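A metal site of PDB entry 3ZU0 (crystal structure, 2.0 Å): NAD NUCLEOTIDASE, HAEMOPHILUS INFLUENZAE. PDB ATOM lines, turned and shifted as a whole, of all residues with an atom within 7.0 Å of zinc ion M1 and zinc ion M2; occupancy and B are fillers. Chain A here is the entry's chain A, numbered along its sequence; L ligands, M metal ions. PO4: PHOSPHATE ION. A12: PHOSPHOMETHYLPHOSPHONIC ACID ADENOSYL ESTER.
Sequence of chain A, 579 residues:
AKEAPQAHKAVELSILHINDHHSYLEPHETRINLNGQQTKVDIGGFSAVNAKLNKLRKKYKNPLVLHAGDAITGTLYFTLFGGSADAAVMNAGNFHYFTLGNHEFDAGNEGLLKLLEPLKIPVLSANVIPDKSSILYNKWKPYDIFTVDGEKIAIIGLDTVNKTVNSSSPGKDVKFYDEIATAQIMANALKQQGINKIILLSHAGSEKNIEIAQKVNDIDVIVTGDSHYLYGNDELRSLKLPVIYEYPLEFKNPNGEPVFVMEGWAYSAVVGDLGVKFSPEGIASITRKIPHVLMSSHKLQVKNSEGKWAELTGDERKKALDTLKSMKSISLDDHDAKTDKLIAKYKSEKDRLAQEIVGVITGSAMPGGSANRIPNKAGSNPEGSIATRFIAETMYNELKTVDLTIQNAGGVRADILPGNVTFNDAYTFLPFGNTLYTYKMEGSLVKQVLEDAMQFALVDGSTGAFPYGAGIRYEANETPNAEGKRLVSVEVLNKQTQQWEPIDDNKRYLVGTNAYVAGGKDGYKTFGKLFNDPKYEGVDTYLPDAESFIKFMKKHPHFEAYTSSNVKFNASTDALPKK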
ATOM      1  N   ASN A  19     -22.068 -32.197  -7.695  1.00  0.00           N
ATOM      2  CA  ASN A  19     -22.228 -30.744  -7.567  1.00  0.00           C
ATOM      3  C   ASN A  19     -20.888 -30.078  -7.430  1.00  0.00           C
ATOM      4  O   ASN A  19     -19.945 -30.674  -6.927  1.00  0.00           O
ATOM      5  CB  ASN A  19     -23.087 -30.412  -6.352  1.00  0.00           C
ATOM      6  CG  ASN A  19     -22.461 -30.916  -5.066  1.00  0.00           C
ATOM      7  OD1 ASN A  19     -22.599 -32.106  -4.721  1.00  0.00           O
ATOM      8  ND2 ASN A  19     -21.743 -30.046  -4.353  1.00  0.00           N
ATOM      9  N   ASP A  20     -20.802 -28.823  -7.855  1.00  0.00           N
ATOM     10  CA  ASP A  20     -19.640 -27.995  -7.594  1.00  0.00           C
ATOM     11  C   ASP A  20     -18.343 -28.670  -8.074  1.00  0.00           C
ATOM     12  O   ASP A  20     -17.334 -28.685  -7.339  1.00  0.00           O
ATOM     13  CB  ASP A  20     -19.528 -27.670  -6.092  1.00  0.00           C
ATOM     14  CG  ASP A  20     -20.687 -26.819  -5.589  1.00  0.00           C
ATOM     15  OD1 ASP A  20     -20.620 -25.579  -5.711  1.00  0.00           O
ATOM     16  OD2 ASP A  20     -21.678 -27.379  -5.085  1.00  0.00           O
ATOM     17  N   HIS A  21     -18.346 -29.205  -9.302  1.00  0.00           N
ATOM     18  CA  HIS A  21     -17.088 -29.814  -9.766  1.00  0.00           C
ATOM     19  C   HIS A  21     -16.084 -28.723 -10.108  1.00  0.00           C
ATOM     20  O   HIS A  21     -14.876 -28.958 -10.084  1.00  0.00           O
ATOM     21  CB  HIS A  21     -17.287 -30.872 -10.860  1.00  0.00           C
ATOM     22  CG  HIS A  21     -17.417 -30.328 -12.248  1.00  0.00           C
ATOM     23  ND1 HIS A  21     -18.643 -30.085 -12.843  1.00  0.00           N
ATOM     24  CD2 HIS A  21     -16.484 -30.063 -13.191  1.00  0.00           C
ATOM     25  CE1 HIS A  21     -18.452 -29.660 -14.079  1.00  0.00           C
ATOM     26  NE2 HIS A  21     -17.149 -29.633 -14.313  1.00  0.00           N
ATOM     27  N   HIS A  22     -16.581 -27.507 -10.373  1.00  0.00           N
ATOM     28  CA  HIS A  22     -15.730 -26.349 -10.568  1.00  0.00           C
ATOM     29  C   HIS A  22     -14.570 -26.581 -11.559  1.00  0.00           C
ATOM     30  O   HIS A  22     -13.443 -26.202 -11.279  1.00  0.00           O
ATOM     31  CB  HIS A  22     -15.157 -25.887  -9.224  1.00  0.00           C
ATOM     32  CG  HIS A  22     -16.109 -25.085  -8.398  1.00  0.00           C
ATOM     33  ND1 HIS A  22     -16.349 -23.746  -8.623  1.00  0.00           N
ATOM     34  CD2 HIS A  22     -16.881 -25.435  -7.335  1.00  0.00           C
ATOM     35  CE1 HIS A  22     -17.234 -23.311  -7.749  1.00  0.00           C
ATOM     36  NE2 HIS A  22     -17.566 -24.310  -6.950  1.00  0.00           N
ATOM     37  N   ALA A  68     -25.876 -30.409  -9.471  1.00  0.00           N
ATOM     38  CA  ALA A  68     -26.502 -29.359  -8.680  1.00  0.00           C
ATOM     39  C   ALA A  68     -25.773 -28.006  -8.742  1.00  0.00           C
ATOM     40  O   ALA A  68     -25.954 -27.181  -7.859  1.00  0.00           O
ATOM     41  CB  ALA A  68     -26.641 -29.808  -7.228  1.00  0.00           C
ATOM     42  N   GLY A  69     -24.941 -27.788  -9.769  1.00  0.00           N
ATOM     43  CA  GLY A  69     -24.427 -26.462 -10.057  1.00  0.00           C
ATOM     44  C   GLY A  69     -22.974 -26.144  -9.754  1.00  0.00           C
ATOM     45  O   GLY A  69     -22.288 -26.907  -9.068  1.00  0.00           O
ATOM     46  N   ASP A  70     -22.507 -24.992 -10.229  1.00  0.00           N
ATOM     47  CA  ASP A  70     -21.074 -24.636 -10.217  1.00  0.00           C
ATOM     48  C   ASP A  70     -20.289 -25.703 -10.968  1.00  0.00           C
ATOM     49  O   ASP A  70     -19.359 -26.304 -10.431  1.00  0.00           O
ATOM     50  CB  ASP A  70     -20.505 -24.486  -8.787  1.00  0.00           C
ATOM     51  CG  ASP A  70     -20.889 -23.191  -8.138  1.00  0.00           C
ATOM     52  OD1 ASP A  70     -21.540 -22.337  -8.777  1.00  0.00           O
ATOM     53  OD2 ASP A  70     -20.472 -23.002  -6.971  1.00  0.00           O
ATOM     54  N   GLY A 101     -25.513 -22.496 -10.632  1.00  0.00           N
ATOM     55  CA  GLY A 101     -24.972 -22.072  -9.357  1.00  0.00           C
ATOM     56  C   GLY A 101     -24.575 -20.605  -9.364  1.00  0.00           C
ATOM     57  O   GLY A 101     -24.918 -19.873 -10.270  1.00  0.00           O
ATOM     58  N   ASN A 102     -23.851 -20.144  -8.341  1.00  0.00           N
ATOM     59  CA  ASN A 102     -23.436 -18.751  -8.325  1.00  0.00           C
ATOM     60  C   ASN A 102     -22.264 -18.482  -9.284  1.00  0.00           C
ATOM     61  O   ASN A 102     -22.236 -17.469  -9.968  1.00  0.00           O
ATOM     62  CB  ASN A 102     -23.096 -18.274  -6.907  1.00  0.00           C
ATOM     63  CG  ASN A 102     -22.158 -19.209  -6.182  1.00  0.00           C
ATOM     64  OD1 ASN A 102     -22.264 -20.419  -6.311  1.00  0.00           O
ATOM     65  ND2 ASN A 102     -21.205 -18.651  -5.440  1.00  0.00           N
ATOM     66  N   HIS A 103     -21.302 -19.399  -9.346  1.00  0.00           N
ATOM     67  CA  HIS A 103     -20.124 -19.206 -10.206  1.00  0.00           C
ATOM     68  C   HIS A 103     -20.390 -19.329 -11.695  1.00  0.00           C
ATOM     69  O   HIS A 103     -19.564 -18.976 -12.506  1.00  0.00           O
ATOM     70  CB  HIS A 103     -18.954 -20.096  -9.769  1.00  0.00           C
ATOM     71  CG  HIS A 103     -18.423 -19.724  -8.425  1.00  0.00           C
ATOM     72  ND1 HIS A 103     -17.487 -18.727  -8.240  1.00  0.00           N
ATOM     73  CD2 HIS A 103     -18.743 -20.170  -7.187  1.00  0.00           C
ATOM     74  CE1 HIS A 103     -17.232 -18.593  -6.951  1.00  0.00           C
ATOM     75  NE2 HIS A 103     -17.980 -19.456  -6.287  1.00  0.00           N
ATOM     76  N   GLU A 104     -21.569 -19.801 -12.049  1.00  0.00           N
ATOM     77  CA  GLU A 104     -21.970 -19.802 -13.465  1.00  0.00           C
ATOM     78  C   GLU A 104     -21.966 -18.402 -14.064  1.00  0.00           C
ATOM     79  O   GLU A 104     -21.804 -18.248 -15.285  1.00  0.00           O
ATOM     80  CB  GLU A 104     -23.373 -20.424 -13.616  1.00  0.00           C
ATOM     81  CG  GLU A 104     -23.379 -21.849 -14.187  1.00  0.00           C
ATOM     82  CD  GLU A 104     -22.828 -22.864 -13.220  1.00  0.00           C
ATOM     83  OE1 GLU A 104     -23.356 -22.973 -12.090  1.00  0.00           O
ATOM     84  OE2 GLU A 104     -21.877 -23.593 -13.590  1.00  0.00           O
ATOM     85  N   ASP A 159     -31.285 -21.347  -7.344  1.00  0.00           N
ATOM     86  CA  ASP A 159     -29.928 -20.831  -7.210  1.00  0.00           C
ATOM     87  C   ASP A 159     -29.848 -20.014  -5.938  1.00  0.00           C
ATOM     88  O   ASP A 159     -30.868 -19.513  -5.438  1.00  0.00           O
ATOM     89  CB  ASP A 159     -29.582 -19.950  -8.412  1.00  0.00           C
ATOM     90  CG  ASP A 159     -28.077 -19.776  -8.620  1.00  0.00           C
ATOM     91  OD1 ASP A 159     -27.268 -20.135  -7.734  1.00  0.00           O
ATOM     92  OD2 ASP A 159     -27.704 -19.254  -9.698  1.00  0.00           O
ATOM     93  N   THR A 160     -28.628 -19.873  -5.421  1.00  0.00           N
ATOM     94  CA  THR A 160     -28.372 -18.972  -4.311  1.00  0.00           C
ATOM     95  C   THR A 160     -28.405 -17.552  -4.860  1.00  0.00           C
ATOM     96  O   THR A 160     -28.020 -17.318  -6.003  1.00  0.00           O
ATOM     97  CB  THR A 160     -27.051 -19.284  -3.592  1.00  0.00           C
ATOM     98  OG1 THR A 160     -26.960 -18.514  -2.386  1.00  0.00           O
ATOM     99  CG2 THR A 160     -25.840 -18.998  -4.483  1.00  0.00           C
ATOM    100  N   LYS A 163     -25.082 -14.286  -2.890  1.00  0.00           N
ATOM    101  CA  LYS A 163     -23.702 -14.526  -3.326  1.00  0.00           C
ATOM    102  C   LYS A 163     -23.555 -14.319  -4.823  1.00  0.00           C
ATOM    103  O   LYS A 163     -22.519 -13.882  -5.290  1.00  0.00           O
ATOM    104  CB  LYS A 163     -23.219 -15.930  -2.960  1.00  0.00           C
ATOM    105  CG  LYS A 163     -22.876 -16.102  -1.482  1.00  0.00           C
ATOM    106  CD  LYS A 163     -22.679 -17.573  -1.111  1.00  0.00           C
ATOM    107  CE  LYS A 163     -21.428 -18.143  -1.716  1.00  0.00           C
ATOM    108  NZ  LYS A 163     -21.210 -19.517  -1.165  1.00  0.00           N
ATOM    109  N   HIS A 203     -28.898 -25.109  -5.758  1.00  0.00           N
ATOM    110  CA  HIS A 203     -27.598 -24.552  -5.402  1.00  0.00           C
ATOM    111  C   HIS A 203     -27.725 -23.466  -4.331  1.00  0.00           C
ATOM    112  O   HIS A 203     -26.886 -22.582  -4.204  1.00  0.00           O
ATOM    113  CB  HIS A 203     -26.900 -23.987  -6.646  1.00  0.00           C
ATOM    114  CG  HIS A 203     -25.417 -23.896  -6.519  1.00  0.00           C
ATOM    115  ND1 HIS A 203     -24.587 -24.964  -6.785  1.00  0.00           N
ATOM    116  CD2 HIS A 203     -24.618 -22.871  -6.147  1.00  0.00           C
ATOM    117  CE1 HIS A 203     -23.333 -24.595  -6.584  1.00  0.00           C
ATOM    118  NE2 HIS A 203     -23.323 -23.325  -6.207  1.00  0.00           N
ATOM    119  N   GLY A 225     -26.327 -28.111  -3.700  1.00  0.00           N
ATOM    120  CA  GLY A 225     -25.035 -27.604  -4.158  1.00  0.00           C
ATOM    121  C   GLY A 225     -24.667 -26.321  -3.424  1.00  0.00           C
ATOM    122  O   GLY A 225     -25.478 -25.776  -2.661  1.00  0.00           O
ATOM    123  N   ASP A 226     -23.433 -25.845  -3.646  1.00  0.00           N
ATOM    124  CA  ASP A 226     -22.918 -24.573  -3.113  1.00  0.00           C
ATOM    125  C   ASP A 226     -22.169 -24.575  -1.778  1.00  0.00           C
ATOM    126  O   ASP A 226     -21.331 -23.703  -1.547  1.00  0.00           O
ATOM    127  CB  ASP A 226     -23.961 -23.446  -3.095  1.00  0.00           C
ATOM    128  CG  ASP A 226     -23.310 -22.082  -2.797  1.00  0.00           C
ATOM    129  OD1 ASP A 226     -22.544 -21.597  -3.644  1.00  0.00           O
ATOM    130  OD2 ASP A 226     -23.538 -21.491  -1.736  1.00  0.00           O
ATOM    131  N   SER A 227     -22.444 -25.523  -0.884  1.00  0.00           N
ATOM    132  CA  SER A 227     -21.719 -25.494   0.375  1.00  0.00           C
ATOM    133  C   SER A 227     -20.463 -26.385   0.355  1.00  0.00           C
ATOM    134  O   SER A 227     -19.589 -26.255   1.212  1.00  0.00           O
ATOM    135  CB  SER A 227     -22.647 -25.811   1.562  1.00  0.00           C
ATOM    136  OG  SER A 227     -23.536 -26.898   1.266  1.00  0.00           O
ATOM    137  N   HIS A 228     -20.367 -27.260  -0.627  1.00  0.00           N
ATOM    138  CA  HIS A 228     -19.196 -28.127  -0.743  1.00  0.00           C
ATOM    139  C   HIS A 228     -19.044 -29.103   0.438  1.00  0.00           C
ATOM    140  O   HIS A 228     -17.939 -29.602   0.673  1.00  0.00           O
ATOM    141  CB  HIS A 228     -17.904 -27.314  -0.900  1.00  0.00           C
ATOM    142  CG  HIS A 228     -17.830 -26.489  -2.146  1.00  0.00           C
ATOM    143  ND1 HIS A 228     -16.641 -25.988  -2.631  1.00  0.00           N
ATOM    144  CD2 HIS A 228     -18.794 -26.057  -3.000  1.00  0.00           C
ATOM    145  CE1 HIS A 228     -16.875 -25.285  -3.728  1.00  0.00           C
ATOM    146  NE2 HIS A 228     -18.174 -25.317  -3.981  1.00  0.00           N
ATOM    147  N   GLU A 263     -25.781 -33.420  -0.203  1.00  0.00           N
ATOM    148  CA  GLU A 263     -24.807 -32.819  -1.106  1.00  0.00           C
ATOM    149  C   GLU A 263     -23.768 -33.892  -1.422  1.00  0.00           C
ATOM    150  O   GLU A 263     -23.732 -34.939  -0.775  1.00  0.00           O
ATOM    151  CB  GLU A 263     -24.122 -31.633  -0.421  1.00  0.00           C
ATOM    152  CG  GLU A 263     -23.267 -30.755  -1.351  1.00  0.00           C
ATOM    153  CD  GLU A 263     -22.991 -29.350  -0.763  1.00  0.00           C
ATOM    154  OE1 GLU A 263     -23.015 -29.171   0.473  1.00  0.00           O
ATOM    155  OE2 GLU A 263     -22.767 -28.417  -1.554  1.00  0.00           O
ATOM    156  N   ALA A 266     -17.485 -31.891  -3.293  1.00  0.00           N
ATOM    157  CA  ALA A 266     -17.156 -30.980  -4.391  1.00  0.00           C
ATOM    158  C   ALA A 266     -15.998 -31.525  -5.218  1.00  0.00           C
ATOM    159  O   ALA A 266     -15.460 -32.586  -4.900  1.00  0.00           O
ATOM    160  CB  ALA A 266     -16.779 -29.591  -3.849  1.00  0.00           C
ATOM    161  N   TYR A 267     -15.626 -30.758  -6.256  1.00  0.00           N
ATOM    162  CA  TYR A 267     -14.428 -31.004  -7.083  1.00  0.00           C
ATOM    163  C   TYR A 267     -14.368 -32.429  -7.668  1.00  0.00           C
ATOM    164  O   TYR A 267     -13.308 -33.061  -7.688  1.00  0.00           O
ATOM    165  CB  TYR A 267     -13.160 -30.687  -6.285  1.00  0.00           C
ATOM    166  CG  TYR A 267     -13.140 -29.307  -5.661  1.00  0.00           C
ATOM    167  CD1 TYR A 267     -13.768 -28.232  -6.276  1.00  0.00           C
ATOM    168  CD2 TYR A 267     -12.525 -29.083  -4.440  1.00  0.00           C
ATOM    169  CE1 TYR A 267     -13.776 -26.964  -5.699  1.00  0.00           C
ATOM    170  CE2 TYR A 267     -12.528 -27.823  -3.843  1.00  0.00           C
ATOM    171  CZ  TYR A 267     -13.152 -26.770  -4.483  1.00  0.00           C
ATOM    172  OH  TYR A 267     -13.158 -25.520  -3.914  1.00  0.00           O
HETATM  173  P   PO4 L   1     -19.074 -21.655  -3.631  1.00  0.00           P
HETATM  174  O1  PO4 L   1     -19.275 -21.947  -2.149  1.00  0.00           O
HETATM  175  O2  PO4 L   1     -20.062 -22.518  -4.405  1.00  0.00           O
HETATM  176  O3  PO4 L   1     -19.433 -20.192  -3.834  1.00  0.00           O
HETATM  177  O4  PO4 L   1     -17.658 -21.957  -4.066  1.00  0.00           O
HETATM  178  PB  A12 L   2     -14.534 -20.246  -4.579  1.00  0.00           P
HETATM  179  O1B A12 L   2     -13.183 -20.735  -3.950  1.00  0.00           O
HETATM  180  O2B A12 L   2     -14.183 -19.578  -5.893  1.00  0.00           O
HETATM  181  O3B A12 L   2     -15.444 -21.374  -4.835  1.00  0.00           O
HETATM  182  PA  A12 L   2     -14.567 -17.531  -3.411  1.00  0.00           P
HETATM  183  O1A A12 L   2     -13.194 -17.692  -4.079  1.00  0.00           O
HETATM  184  O2A A12 L   2     -14.608 -16.797  -2.046  1.00  0.00           O
HETATM  185  C3A A12 L   2     -15.260 -19.079  -3.571  1.00  0.00           C
HETATM  186  O5' A12 L   2     -15.446 -16.918  -4.640  1.00  0.00           O
HETATM  187  C5' A12 L   2     -15.893 -15.603  -4.548  1.00  0.00           C
HETATM  188  C4' A12 L   2     -14.910 -14.565  -4.572  1.00  0.00           C
HETATM  189  O4' A12 L   2     -14.288 -14.575  -5.890  1.00  0.00           O
HETATM  190  C3' A12 L   2     -15.528 -13.232  -4.576  1.00  0.00           C
HETATM  191  O3' A12 L   2     -15.898 -12.785  -3.336  1.00  0.00           O
HETATM  192  C2' A12 L   2     -14.492 -12.364  -5.201  1.00  0.00           C
HETATM  193  O2' A12 L   2     -13.582 -11.925  -4.270  1.00  0.00           O
HETATM  194  C1' A12 L   2     -13.858 -13.274  -6.187  1.00  0.00           C
HETATM  195  N9  A12 L   2     -14.274 -12.918  -7.523  1.00  0.00           N
HETATM  196  C8  A12 L   2     -15.323 -13.445  -8.202  1.00  0.00           C
HETATM  197  N7  A12 L   2     -15.365 -12.833  -9.382  1.00  0.00           N
HETATM  198  C5  A12 L   2     -14.328 -11.917  -9.469  1.00  0.00           C
HETATM  199  C6  A12 L   2     -13.878 -11.009 -10.463  1.00  0.00           C
HETATM  200  N6  A12 L   2     -14.507 -10.862 -11.707  1.00  0.00           N
HETATM  201  N1  A12 L   2     -12.808 -10.274 -10.204  1.00  0.00           N
HETATM  202  C2  A12 L   2     -12.181 -10.353  -9.039  1.00  0.00           C
HETATM  203  N3  A12 L   2     -12.570 -11.192  -8.067  1.00  0.00           N
HETATM  204  C4  A12 L   2     -13.641 -11.970  -8.276  1.00  0.00           C
HETATM  205 ZN    ZN M   1     -21.735 -22.244  -5.525  1.00  0.00          ZN
HETATM  206 ZN    ZN M   2     -19.086 -24.174  -5.478  1.00  0.00          ZN
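Of the 22 residues printed, 5 come within 4 Å of zinc ion M1.
The nearest printed residue that does not touch zinc ion M1 is His 103 (4.002 Å).
Zinc ion M1 is bound by an oxygen (O2) of PO4 L1 (2.0 Å), a ring nitrogen (NE2) of His 203 (2.0 Å), the side-chain amide oxygen of Asn 102 (2.1 Å), the side-chain carboxylate of Asp 70 (2.1 Å) and the side-chain carboxylate of Asp 226 (2.1 Å).
Zinc ion M1 has five donor atoms within binding distance.
The backbone carbonyl oxygen of Asp 20 is in hydrogen-bond range of the backbone NH of Tyr 267, 2.9 Å away.
The side-chain carboxylate of Asp 70 is in hydrogen-bond range of the backbone NH of His 103 (3.0 Å).
The side-chain amide nitrogen (ND2) of Asn 102 lies close to a ring nitrogen (NE2) of His 103 (3.4 Å).
The backbone carbonyl oxygen of His 203 sits close to the backbone NH of Thr 160 (3.4 Å).
The side-chain amide nitrogen (ND2) of Asn 19 is in hydrogen-bond range of the side-chain carboxylate (OD2) of Asp 20 (2.8 Å).
The backbone NH (N) of Asn 102 is in hydrogen-bond range of the side-chain carboxylate (OD1) of Asp 159, 3.5 Å away.
The backbone carbonyl oxygen (O) of Gly 69 sits at hydrogen-bond distance from the backbone NH (N) of Asp 20 (2.7 Å).
The backbone NH (N) of Asp 70 is in hydrogen-bond range of the side-chain carboxylate (OE1) of Glu 104 (2.9 Å).
NE2 of His 228 binds zinc ion M2 (2.1 Å).
OD1 of Asp 20 binds zinc ion M2.
A ring nitrogen (NE2) of His 22 binds zinc ion M2 (2.1 Å).
O2 of PO4 L1 is bound to zinc ion M2.
Zinc ion M2 is bound by the side-chain carboxylate (OD2) of Asp 70.
Zinc ion M2 has five donor atoms within binding distance.
Of the 22 residues printed, 4 come within 4 Å of zinc ion M2.
Along chain A the residues within 4 Å of zinc ion M2 span positions 20 to 228.
An oxygen (O3B) of A12 L2 is in hydrogen-bond range of a ring nitrogen (NE2) of His 103, at 3.5 Å.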
